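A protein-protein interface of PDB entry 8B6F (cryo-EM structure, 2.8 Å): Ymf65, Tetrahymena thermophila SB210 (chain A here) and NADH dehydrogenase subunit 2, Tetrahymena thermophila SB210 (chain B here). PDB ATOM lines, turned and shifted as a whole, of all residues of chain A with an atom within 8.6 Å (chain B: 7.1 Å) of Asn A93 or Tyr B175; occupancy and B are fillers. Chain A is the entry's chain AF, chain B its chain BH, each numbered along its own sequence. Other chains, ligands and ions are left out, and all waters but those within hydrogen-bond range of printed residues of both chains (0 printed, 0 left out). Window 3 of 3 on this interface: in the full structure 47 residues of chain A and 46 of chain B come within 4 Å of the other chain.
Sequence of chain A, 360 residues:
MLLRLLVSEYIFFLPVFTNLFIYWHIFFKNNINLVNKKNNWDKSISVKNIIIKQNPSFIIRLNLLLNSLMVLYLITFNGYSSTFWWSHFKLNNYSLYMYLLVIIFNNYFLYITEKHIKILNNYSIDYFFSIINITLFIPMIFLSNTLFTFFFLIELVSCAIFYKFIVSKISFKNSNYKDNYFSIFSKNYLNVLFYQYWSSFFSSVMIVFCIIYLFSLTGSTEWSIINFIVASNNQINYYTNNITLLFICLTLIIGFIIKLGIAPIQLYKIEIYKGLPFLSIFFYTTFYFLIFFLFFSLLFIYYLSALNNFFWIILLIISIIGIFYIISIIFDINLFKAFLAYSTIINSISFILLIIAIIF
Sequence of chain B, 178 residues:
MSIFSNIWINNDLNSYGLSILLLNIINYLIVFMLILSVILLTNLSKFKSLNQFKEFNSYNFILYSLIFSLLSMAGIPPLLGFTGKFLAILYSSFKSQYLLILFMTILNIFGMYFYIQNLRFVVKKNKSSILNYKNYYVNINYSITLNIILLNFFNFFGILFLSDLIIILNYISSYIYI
Of chain B, only Tyr B175 (3.3 Å) comes within 4 Å of Asn A93.
Of chain A, only Asn A93, Tyr A94 and Tyr A97 come within 4 Å of Tyr B175.
No residue of chain A comes within 4 Å of Ser B174.
Printed residues of chain B within 4 Å of Tyr A97: Tyr B171, Ile B172 and Tyr B175.
Of the printed residues of chain A, Ile B176 touches Tyr A94 (3.7 Å) and Tyr A302 (3.4 Å).
The nearest residue of chain B that does not touch Asn A93 is Ile B172 (5.9 Å).
The nearest residue of chain A that does not touch Tyr B175 is Asn A92 (6.4 Å).
Among the printed residues, merely in contact across the chains: Asn A93 with Tyr B175 (3.3 Å), Tyr A302 with Ile B176 (3.4 Å), Tyr A302 with Ile B178 (3.5 Å), Tyr A94 with Ile B172 (3.5 Å), Tyr A97 with Tyr B175 (3.6 Å), Tyr A94 with Ile B176 (3.7 Å), Tyr A97 with Ile B172 (3.9 Å) and Tyr A94 with Tyr B175 (3.9 Å).
The side-chain hydroxyl (OH) of Tyr B175 sits at hydrogen-bond distance from the side-chain hydroxyl (OH) of Tyr B171 (3.0 Å).
OH of Tyr A94 sits at hydrogen-bond distance from SD of Met A98 (3.2 Å).
O of Tyr B171 is in hydrogen-bond range of OG of Ser B174, 2.7 Å away.
Printed residues of chain B that touch a printed residue of chain A: Tyr B171, Ile B172, Tyr B175, Ile B176 and Ile B178.
Of the 19 printed residues of chain A, 4 touch a printed residue of chain B.
Hydrophobic or aromatic side chains of chain A that line the printed part of chain B: Tyr A94, Tyr A97 and Tyr A302.
Among the printed residues, no Asp or Glu carboxylate lies within 4 Å of a Lys or Arg side-chain nitrogen of the other chain.
The side-chain hydroxyl (OH) of Tyr A97 lies within hydrogen-bond range of the side-chain hydroxyl (OH) of Tyr B171.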
ATOM      1  N   PHE A  77       4.999  15.241  11.907  1.00  0.00           N
ATOM      2  CA  PHE A  77       6.119  14.774  11.104  1.00  0.00           C
ATOM      3  C   PHE A  77       6.030  15.298   9.675  1.00  0.00           C
ATOM      4  O   PHE A  77       4.946  15.473   9.117  1.00  0.00           O
ATOM      5  CB  PHE A  77       6.158  13.245  11.101  1.00  0.00           C
ATOM      6  CG  PHE A  77       7.403  12.675  10.496  1.00  0.00           C
ATOM      7  CD1 PHE A  77       8.526  12.459  11.274  1.00  0.00           C
ATOM      8  CD2 PHE A  77       7.452  12.354   9.152  1.00  0.00           C
ATOM      9  CE1 PHE A  77       9.674  11.935  10.724  1.00  0.00           C
ATOM     10  CE2 PHE A  77       8.600  11.830   8.596  1.00  0.00           C
ATOM     11  CZ  PHE A  77       9.711  11.620   9.384  1.00  0.00           C
ATOM     12  N   ASN A  78       7.200  15.551   9.089  1.00  0.00           N
ATOM     13  CA  ASN A  78       7.316  15.959   7.695  1.00  0.00           C
ATOM     14  C   ASN A  78       8.594  15.361   7.125  1.00  0.00           C
ATOM     15  O   ASN A  78       9.513  14.998   7.860  1.00  0.00           O
ATOM     16  CB  ASN A  78       7.342  17.485   7.545  1.00  0.00           C
ATOM     17  CG  ASN A  78       6.042  18.136   7.958  1.00  0.00           C
ATOM     18  OD1 ASN A  78       4.961  17.628   7.672  1.00  0.00           O
ATOM     19  ND2 ASN A  78       6.140  19.270   8.637  1.00  0.00           N
ATOM     20  N   GLY A  79       8.642  15.260   5.809  1.00  0.00           N
ATOM     21  CA  GLY A  79       9.834  14.779   5.139  1.00  0.00           C
ATOM     22  C   GLY A  79       9.493  14.176   3.793  1.00  0.00           C
ATOM     23  O   GLY A  79       8.340  14.124   3.379  1.00  0.00           O
ATOM     24  N   TYR A  80      10.542  13.728   3.109  1.00  0.00           N
ATOM     25  CA  TYR A  80      10.400  12.999   1.858  1.00  0.00           C
ATOM     26  C   TYR A  80      10.237  11.512   2.141  1.00  0.00           C
ATOM     27  O   TYR A  80      10.701  11.000   3.163  1.00  0.00           O
ATOM     28  CB  TYR A  80      11.614  13.211   0.953  1.00  0.00           C
ATOM     29  CG  TYR A  80      11.884  14.650   0.582  1.00  0.00           C
ATOM     30  CD1 TYR A  80      11.164  15.277  -0.426  1.00  0.00           C
ATOM     31  CD2 TYR A  80      12.879  15.372   1.223  1.00  0.00           C
ATOM     32  CE1 TYR A  80      11.418  16.589  -0.772  1.00  0.00           C
ATOM     33  CE2 TYR A  80      13.142  16.681   0.885  1.00  0.00           C
ATOM     34  CZ  TYR A  80      12.409  17.284  -0.113  1.00  0.00           C
ATOM     35  OH  TYR A  80      12.674  18.590  -0.446  1.00  0.00           O
ATOM     36  N   SER A  81       9.576  10.818   1.221  1.00  0.00           N
ATOM     37  CA  SER A  81       9.417   9.373   1.325  1.00  0.00           C
ATOM     38  C   SER A  81      10.668   8.710   0.762  1.00  0.00           C
ATOM     39  O   SER A  81      10.901   8.738  -0.450  1.00  0.00           O
ATOM     40  CB  SER A  81       8.163   8.910   0.588  1.00  0.00           C
ATOM     41  OG  SER A  81       8.264   9.162  -0.801  1.00  0.00           O
ATOM     42  N   SER A  82      11.477   8.125   1.636  1.00  0.00           N
ATOM     43  CA  SER A  82      12.729   7.492   1.233  1.00  0.00           C
ATOM     44  C   SER A  82      13.250   6.686   2.415  1.00  0.00           C
ATOM     45  O   SER A  82      12.602   6.587   3.462  1.00  0.00           O
ATOM     46  CB  SER A  82      13.756   8.529   0.772  1.00  0.00           C
ATOM     47  OG  SER A  82      13.287   9.254  -0.352  1.00  0.00           O
ATOM     48  N   LYS A  90      12.946   2.327   6.238  1.00  0.00           N
ATOM     49  CA  LYS A  90      12.103   2.954   5.232  1.00  0.00           C
ATOM     50  C   LYS A  90      11.199   3.986   5.889  1.00  0.00           C
ATOM     51  O   LYS A  90      10.666   3.756   6.978  1.00  0.00           O
ATOM     52  CB  LYS A  90      11.260   1.911   4.494  1.00  0.00           C
ATOM     53  CG  LYS A  90      10.249   2.492   3.505  1.00  0.00           C
ATOM     54  CD  LYS A  90      10.910   3.296   2.392  1.00  0.00           C
ATOM     55  CE  LYS A  90      11.605   2.404   1.379  1.00  0.00           C
ATOM     56  NZ  LYS A  90      10.639   1.572   0.610  1.00  0.00           N
ATOM     57  N   LEU A  91      11.032   5.124   5.221  1.00  0.00           N
ATOM     58  CA  LEU A  91      10.242   6.245   5.729  1.00  0.00           C
ATOM     59  C   LEU A  91       9.220   6.607   4.656  1.00  0.00           C
ATOM     60  O   LEU A  91       9.513   7.399   3.760  1.00  0.00           O
ATOM     61  CB  LEU A  91      11.147   7.422   6.069  1.00  0.00           C
ATOM     62  CG  LEU A  91      10.512   8.579   6.833  1.00  0.00           C
ATOM     63  CD1 LEU A  91      10.286   8.183   8.282  1.00  0.00           C
ATOM     64  CD2 LEU A  91      11.387   9.816   6.730  1.00  0.00           C
ATOM     65  N   ASN A  92       8.027   6.023   4.741  1.00  0.00           N
ATOM     66  CA  ASN A  92       6.965   6.305   3.787  1.00  0.00           C
ATOM     67  C   ASN A  92       5.631   6.332   4.518  1.00  0.00           C
ATOM     68  O   ASN A  92       5.537   6.001   5.702  1.00  0.00           O
ATOM     69  CB  ASN A  92       6.942   5.283   2.642  1.00  0.00           C
ATOM     70  CG  ASN A  92       6.790   3.860   3.128  1.00  0.00           C
ATOM     71  OD1 ASN A  92       6.449   3.619   4.282  1.00  0.00           O
ATOM     72  ND2 ASN A  92       7.035   2.905   2.241  1.00  0.00           N
ATOM     73  N   ASN A  93       4.589   6.737   3.790  1.00  0.00           N
ATOM     74  CA  ASN A  93       3.297   6.992   4.418  1.00  0.00           C
ATOM     75  C   ASN A  93       2.729   5.736   5.066  1.00  0.00           C
ATOM     76  O   ASN A  93       2.232   5.785   6.196  1.00  0.00           O
ATOM     77  CB  ASN A  93       2.318   7.551   3.388  1.00  0.00           C
ATOM     78  CG  ASN A  93       2.732   8.915   2.878  1.00  0.00           C
ATOM     79  OD1 ASN A  93       3.250   9.738   3.627  1.00  0.00           O
ATOM     80  ND2 ASN A  93       2.508   9.161   1.596  1.00  0.00           N
ATOM     81  N   TYR A  94       2.785   4.600   4.369  1.00  0.00           N
ATOM     82  CA  TYR A  94       2.198   3.381   4.917  1.00  0.00           C
ATOM     83  C   TYR A  94       2.949   2.910   6.154  1.00  0.00           C
ATOM     84  O   TYR A  94       2.331   2.537   7.157  1.00  0.00           O
ATOM     85  CB  TYR A  94       2.174   2.273   3.866  1.00  0.00           C
ATOM     86  CG  TYR A  94       1.583   0.990   4.400  1.00  0.00           C
ATOM     87  CD1 TYR A  94       0.209   0.820   4.489  1.00  0.00           C
ATOM     88  CD2 TYR A  94       2.401  -0.048   4.827  1.00  0.00           C
ATOM     89  CE1 TYR A  94      -0.335  -0.347   4.985  1.00  0.00           C
ATOM     90  CE2 TYR A  94       1.869  -1.218   5.325  1.00  0.00           C
ATOM     91  CZ  TYR A  94       0.499  -1.361   5.401  1.00  0.00           C
ATOM     92  OH  TYR A  94      -0.038  -2.526   5.894  1.00  0.00           O
ATOM     93  N   SER A  95       4.281   2.922   6.109  1.00  0.00           N
ATOM     94  CA  SER A  95       5.058   2.497   7.266  1.00  0.00           C
ATOM     95  C   SER A  95       4.801   3.405   8.461  1.00  0.00           C
ATOM     96  O   SER A  95       4.658   2.929   9.593  1.00  0.00           O
ATOM     97  CB  SER A  95       6.543   2.484   6.915  1.00  0.00           C
ATOM     98  OG  SER A  95       7.313   1.968   7.982  1.00  0.00           O
ATOM     99  N   LEU A  96       4.746   4.716   8.231  1.00  0.00           N
ATOM    100  CA  LEU A  96       4.477   5.646   9.321  1.00  0.00           C
ATOM    101  C   LEU A  96       3.079   5.446   9.889  1.00  0.00           C
ATOM    102  O   LEU A  96       2.880   5.531  11.106  1.00  0.00           O
ATOM    103  CB  LEU A  96       4.672   7.086   8.846  1.00  0.00           C
ATOM    104  CG  LEU A  96       6.123   7.464   8.534  1.00  0.00           C
ATOM    105  CD1 LEU A  96       6.200   8.836   7.901  1.00  0.00           C
ATOM    106  CD2 LEU A  96       6.975   7.422   9.794  1.00  0.00           C
ATOM    107  N   TYR A  97       2.097   5.166   9.031  1.00  0.00           N
ATOM    108  CA  TYR A  97       0.749   4.914   9.528  1.00  0.00           C
ATOM    109  C   TYR A  97       0.703   3.646  10.366  1.00  0.00           C
ATOM    110  O   TYR A  97      -0.001   3.594  11.380  1.00  0.00           O
ATOM    111  CB  TYR A  97      -0.230   4.830   8.360  1.00  0.00           C
ATOM    112  CG  TYR A  97      -0.884   6.155   8.078  1.00  0.00           C
ATOM    113  CD1 TYR A  97      -1.854   6.675   8.926  1.00  0.00           C
ATOM    114  CD2 TYR A  97      -0.506   6.904   6.977  1.00  0.00           C
ATOM    115  CE1 TYR A  97      -2.442   7.897   8.668  1.00  0.00           C
ATOM    116  CE2 TYR A  97      -1.079   8.119   6.714  1.00  0.00           C
ATOM    117  CZ  TYR A  97      -2.035   8.618   7.565  1.00  0.00           C
ATOM    118  OH  TYR A  97      -2.586   9.834   7.267  1.00  0.00           O
ATOM    119  N   MET A  98       1.433   2.608   9.959  1.00  0.00           N
ATOM    120  CA  MET A  98       1.514   1.412  10.789  1.00  0.00           C
ATOM    121  C   MET A  98       2.130   1.741  12.141  1.00  0.00           C
ATOM    122  O   MET A  98       1.643   1.288  13.182  1.00  0.00           O
ATOM    123  CB  MET A  98       2.324   0.328  10.080  1.00  0.00           C
ATOM    124  CG  MET A  98       1.744  -0.142   8.748  1.00  0.00           C
ATOM    125  SD  MET A  98       0.415  -1.362   8.859  1.00  0.00           S
ATOM    126  CE  MET A  98      -1.015  -0.360   9.273  1.00  0.00           C
ATOM    127  N   TYR A  99       3.210   2.523  12.142  1.00  0.00           N
ATOM    128  CA  TYR A  99       3.825   2.942  13.396  1.00  0.00           C
ATOM    129  C   TYR A  99       2.813   3.669  14.273  1.00  0.00           C
ATOM    130  O   TYR A  99       2.681   3.378  15.468  1.00  0.00           O
ATOM    131  CB  TYR A  99       5.030   3.837  13.099  1.00  0.00           C
ATOM    132  CG  TYR A  99       5.996   4.006  14.248  1.00  0.00           C
ATOM    133  CD1 TYR A  99       5.676   4.788  15.348  1.00  0.00           C
ATOM    134  CD2 TYR A  99       7.246   3.405  14.214  1.00  0.00           C
ATOM    135  CE1 TYR A  99       6.567   4.950  16.392  1.00  0.00           C
ATOM    136  CE2 TYR A  99       8.142   3.561  15.248  1.00  0.00           C
ATOM    137  CZ  TYR A  99       7.798   4.333  16.335  1.00  0.00           C
ATOM    138  OH  TYR A  99       8.692   4.488  17.369  1.00  0.00           O
ATOM    139  N   LEU A 100       2.078   4.614  13.686  1.00  0.00           N
ATOM    140  CA  LEU A 100       1.113   5.398  14.451  1.00  0.00           C
ATOM    141  C   LEU A 100      -0.010   4.523  14.993  1.00  0.00           C
ATOM    142  O   LEU A 100      -0.439   4.691  16.139  1.00  0.00           O
ATOM    143  CB  LEU A 100       0.546   6.523  13.583  1.00  0.00           C
ATOM    144  CG  LEU A 100      -0.523   7.407  14.230  1.00  0.00           C
ATOM    145  CD1 LEU A 100       0.003   8.083  15.485  1.00  0.00           C
ATOM    146  CD2 LEU A 100      -1.018   8.443  13.238  1.00  0.00           C
ATOM    147  N   LEU A 143       9.110   0.081  10.349  1.00  0.00           N
ATOM    148  CA  LEU A 143      10.064   0.940   9.663  1.00  0.00           C
ATOM    149  C   LEU A 143      11.235   0.161   9.082  1.00  0.00           C
ATOM    150  O   LEU A 143      12.107   0.762   8.447  1.00  0.00           O
ATOM    151  CB  LEU A 143      10.582   2.019  10.619  1.00  0.00           C
ATOM    152  CG  LEU A 143       9.531   3.024  11.099  1.00  0.00           C
ATOM    153  CD1 LEU A 143      10.058   3.820  12.276  1.00  0.00           C
ATOM    154  CD2 LEU A 143       9.117   3.956   9.973  1.00  0.00           C
ATOM    155  N   TYR A 302       3.248  -7.539   0.801  1.00  0.00           N
ATOM    156  CA  TYR A 302       4.014  -6.350   0.448  1.00  0.00           C
ATOM    157  C   TYR A 302       5.510  -6.596   0.351  1.00  0.00           C
ATOM    158  O   TYR A 302       6.131  -6.197  -0.641  1.00  0.00           O
ATOM    159  CB  TYR A 302       3.734  -5.248   1.482  1.00  0.00           C
ATOM    160  CG  TYR A 302       4.603  -4.018   1.359  1.00  0.00           C
ATOM    161  CD1 TYR A 302       4.595  -3.250   0.202  1.00  0.00           C
ATOM    162  CD2 TYR A 302       5.392  -3.598   2.419  1.00  0.00           C
ATOM    163  CE1 TYR A 302       5.373  -2.114   0.095  1.00  0.00           C
ATOM    164  CE2 TYR A 302       6.173  -2.466   2.322  1.00  0.00           C
ATOM    165  CZ  TYR A 302       6.159  -1.726   1.159  1.00  0.00           C
ATOM    166  OH  TYR A 302       6.936  -0.596   1.063  1.00  0.00           O
ATOM    167  N   SER B  15      -5.718  -2.196  -3.438  1.00  0.00           N
ATOM    168  CA  SER B  15      -5.466  -2.004  -2.011  1.00  0.00           C
ATOM    169  C   SER B  15      -6.776  -2.074  -1.225  1.00  0.00           C
ATOM    170  O   SER B  15      -7.183  -1.137  -0.539  1.00  0.00           O
ATOM    171  CB  SER B  15      -4.765  -0.673  -1.785  1.00  0.00           C
ATOM    172  OG  SER B  15      -5.592   0.394  -2.216  1.00  0.00           O
ATOM    173  N   ASN B 170      -8.975   1.855   3.992  1.00  0.00           N
ATOM    174  CA  ASN B 170      -8.608   1.886   2.580  1.00  0.00           C
ATOM    175  C   ASN B 170      -7.686   3.059   2.282  1.00  0.00           C
ATOM    176  O   ASN B 170      -6.765   2.947   1.468  1.00  0.00           O
ATOM    177  CB  ASN B 170      -9.861   1.958   1.712  1.00  0.00           C
ATOM    178  CG  ASN B 170     -10.527   0.612   1.549  1.00  0.00           C
ATOM    179  OD1 ASN B 170     -10.300  -0.086   0.564  1.00  0.00           O
ATOM    180  ND2 ASN B 170     -11.351   0.235   2.519  1.00  0.00           N
ATOM    181  N   TYR B 171      -7.931   4.198   2.926  1.00  0.00           N
ATOM    182  CA  TYR B 171      -7.043   5.341   2.772  1.00  0.00           C
ATOM    183  C   TYR B 171      -5.635   5.011   3.251  1.00  0.00           C
ATOM    184  O   TYR B 171      -4.648   5.376   2.603  1.00  0.00           O
ATOM    185  CB  TYR B 171      -7.621   6.531   3.530  1.00  0.00           C
ATOM    186  CG  TYR B 171      -6.608   7.542   3.980  1.00  0.00           C
ATOM    187  CD1 TYR B 171      -6.090   8.466   3.090  1.00  0.00           C
ATOM    188  CD2 TYR B 171      -6.193   7.595   5.301  1.00  0.00           C
ATOM    189  CE1 TYR B 171      -5.176   9.400   3.494  1.00  0.00           C
ATOM    190  CE2 TYR B 171      -5.277   8.527   5.716  1.00  0.00           C
ATOM    191  CZ  TYR B 171      -4.780   9.432   4.808  1.00  0.00           C
ATOM    192  OH  TYR B 171      -3.866  10.362   5.218  1.00  0.00           O
ATOM    193  N   ILE B 172      -5.522   4.325   4.390  1.00  0.00           N
ATOM    194  CA  ILE B 172      -4.211   3.947   4.911  1.00  0.00           C
ATOM    195  C   ILE B 172      -3.522   2.972   3.965  1.00  0.00           C
ATOM    196  O   ILE B 172      -2.322   3.090   3.694  1.00  0.00           O
ATOM    197  CB  ILE B 172      -4.352   3.361   6.328  1.00  0.00           C
ATOM    198  CG1 ILE B 172      -4.790   4.455   7.305  1.00  0.00           C
ATOM    199  CG2 ILE B 172      -3.044   2.719   6.786  1.00  0.00           C
ATOM    200  CD1 ILE B 172      -5.171   3.944   8.675  1.00  0.00           C
ATOM    201  N   SER B 173      -4.266   1.990   3.457  1.00  0.00           N
ATOM    202  CA  SER B 173      -3.654   0.953   2.633  1.00  0.00           C
ATOM    203  C   SER B 173      -3.318   1.461   1.237  1.00  0.00           C
ATOM    204  O   SER B 173      -2.411   0.927   0.592  1.00  0.00           O
ATOM    205  CB  SER B 173      -4.576  -0.262   2.546  1.00  0.00           C
ATOM    206  OG  SER B 173      -5.792   0.063   1.897  1.00  0.00           O
ATOM    207  N   SER B 174      -4.022   2.486   0.754  1.00  0.00           N
ATOM    208  CA  SER B 174      -3.774   2.968  -0.600  1.00  0.00           C
ATOM    209  C   SER B 174      -2.363   3.508  -0.763  1.00  0.00           C
ATOM    210  O   SER B 174      -1.854   3.545  -1.888  1.00  0.00           O
ATOM    211  CB  SER B 174      -4.789   4.048  -0.974  1.00  0.00           C
ATOM    212  OG  SER B 174      -4.669   5.180  -0.133  1.00  0.00           O
ATOM    213  N   TYR B 175      -1.718   3.929   0.325  1.00  0.00           N
ATOM    214  CA  TYR B 175      -0.342   4.399   0.220  1.00  0.00           C
ATOM    215  C   TYR B 175       0.589   3.280  -0.216  1.00  0.00           C
ATOM    216  O   TYR B 175       1.564   3.528  -0.933  1.00  0.00           O
ATOM    217  CB  TYR B 175       0.121   4.988   1.550  1.00  0.00           C
ATOM    218  CG  TYR B 175      -0.518   6.312   1.874  1.00  0.00           C
ATOM    219  CD1 TYR B 175      -0.256   7.432   1.098  1.00  0.00           C
ATOM    220  CD2 TYR B 175      -1.372   6.450   2.957  1.00  0.00           C
ATOM    221  CE1 TYR B 175      -0.830   8.648   1.385  1.00  0.00           C
ATOM    222  CE2 TYR B 175      -1.952   7.663   3.254  1.00  0.00           C
ATOM    223  CZ  TYR B 175      -1.674   8.759   2.465  1.00  0.00           C
ATOM    224  OH  TYR B 175      -2.246   9.973   2.753  1.00  0.00           O
ATOM    225  N   ILE B 176       0.309   2.051   0.208  1.00  0.00           N
ATOM    226  CA  ILE B 176       1.080   0.908  -0.257  1.00  0.00           C
ATOM    227  C   ILE B 176       0.825   0.741  -1.748  1.00  0.00           C
ATOM    228  O   ILE B 176      -0.329   0.694  -2.196  1.00  0.00           O
ATOM    229  CB  ILE B 176       0.702  -0.346   0.548  1.00  0.00           C
ATOM    230  CG1 ILE B 176       1.952  -1.155   0.891  1.00  0.00           C
ATOM    231  CG2 ILE B 176      -0.289  -1.234  -0.212  1.00  0.00           C
ATOM    232  CD1 ILE B 176       1.676  -2.306   1.840  1.00  0.00           C
ATOM    233  N   TYR B 177       1.900   0.676  -2.530  1.00  0.00           N
ATOM    234  CA  TYR B 177       1.795   0.528  -3.980  1.00  0.00           C
ATOM    235  C   TYR B 177       1.991  -0.942  -4.337  1.00  0.00           C
ATOM    236  O   TYR B 177       3.051  -1.375  -4.788  1.00  0.00           O
ATOM    237  CB  TYR B 177       2.798   1.435  -4.681  1.00  0.00           C
ATOM    238  CG  TYR B 177       2.487   2.899  -4.496  1.00  0.00           C
ATOM    239  CD1 TYR B 177       1.392   3.481  -5.123  1.00  0.00           C
ATOM    240  CD2 TYR B 177       3.281   3.701  -3.687  1.00  0.00           C
ATOM    241  CE1 TYR B 177       1.097   4.818  -4.953  1.00  0.00           C
ATOM    242  CE2 TYR B 177       2.996   5.040  -3.510  1.00  0.00           C
ATOM    243  CZ  TYR B 177       1.902   5.592  -4.146  1.00  0.00           C
ATOM    244  OH  TYR B 177       1.613   6.925  -3.974  1.00  0.00           O
ATOM    245  N   ILE B 178       0.935  -1.717  -4.112  1.00  0.00           N
ATOM    246  CA  ILE B 178       0.935  -3.140  -4.406  1.00  0.00           C
ATOM    247  C   ILE B 178      -0.324  -3.465  -5.196  1.00  0.00           C
ATOM    248  O   ILE B 178      -1.374  -2.855  -4.988  1.00  0.00           O
ATOM    249  CB  ILE B 178       1.009  -3.977  -3.120  1.00  0.00           C
ATOM    250  CG1 ILE B 178       2.303  -3.677  -2.359  1.00  0.00           C
ATOM    251  CG2 ILE B 178       0.894  -5.470  -3.436  1.00  0.00           C
ATOM    252  CD1 ILE B 178       3.556  -4.063  -3.092  1.00  0.00           C
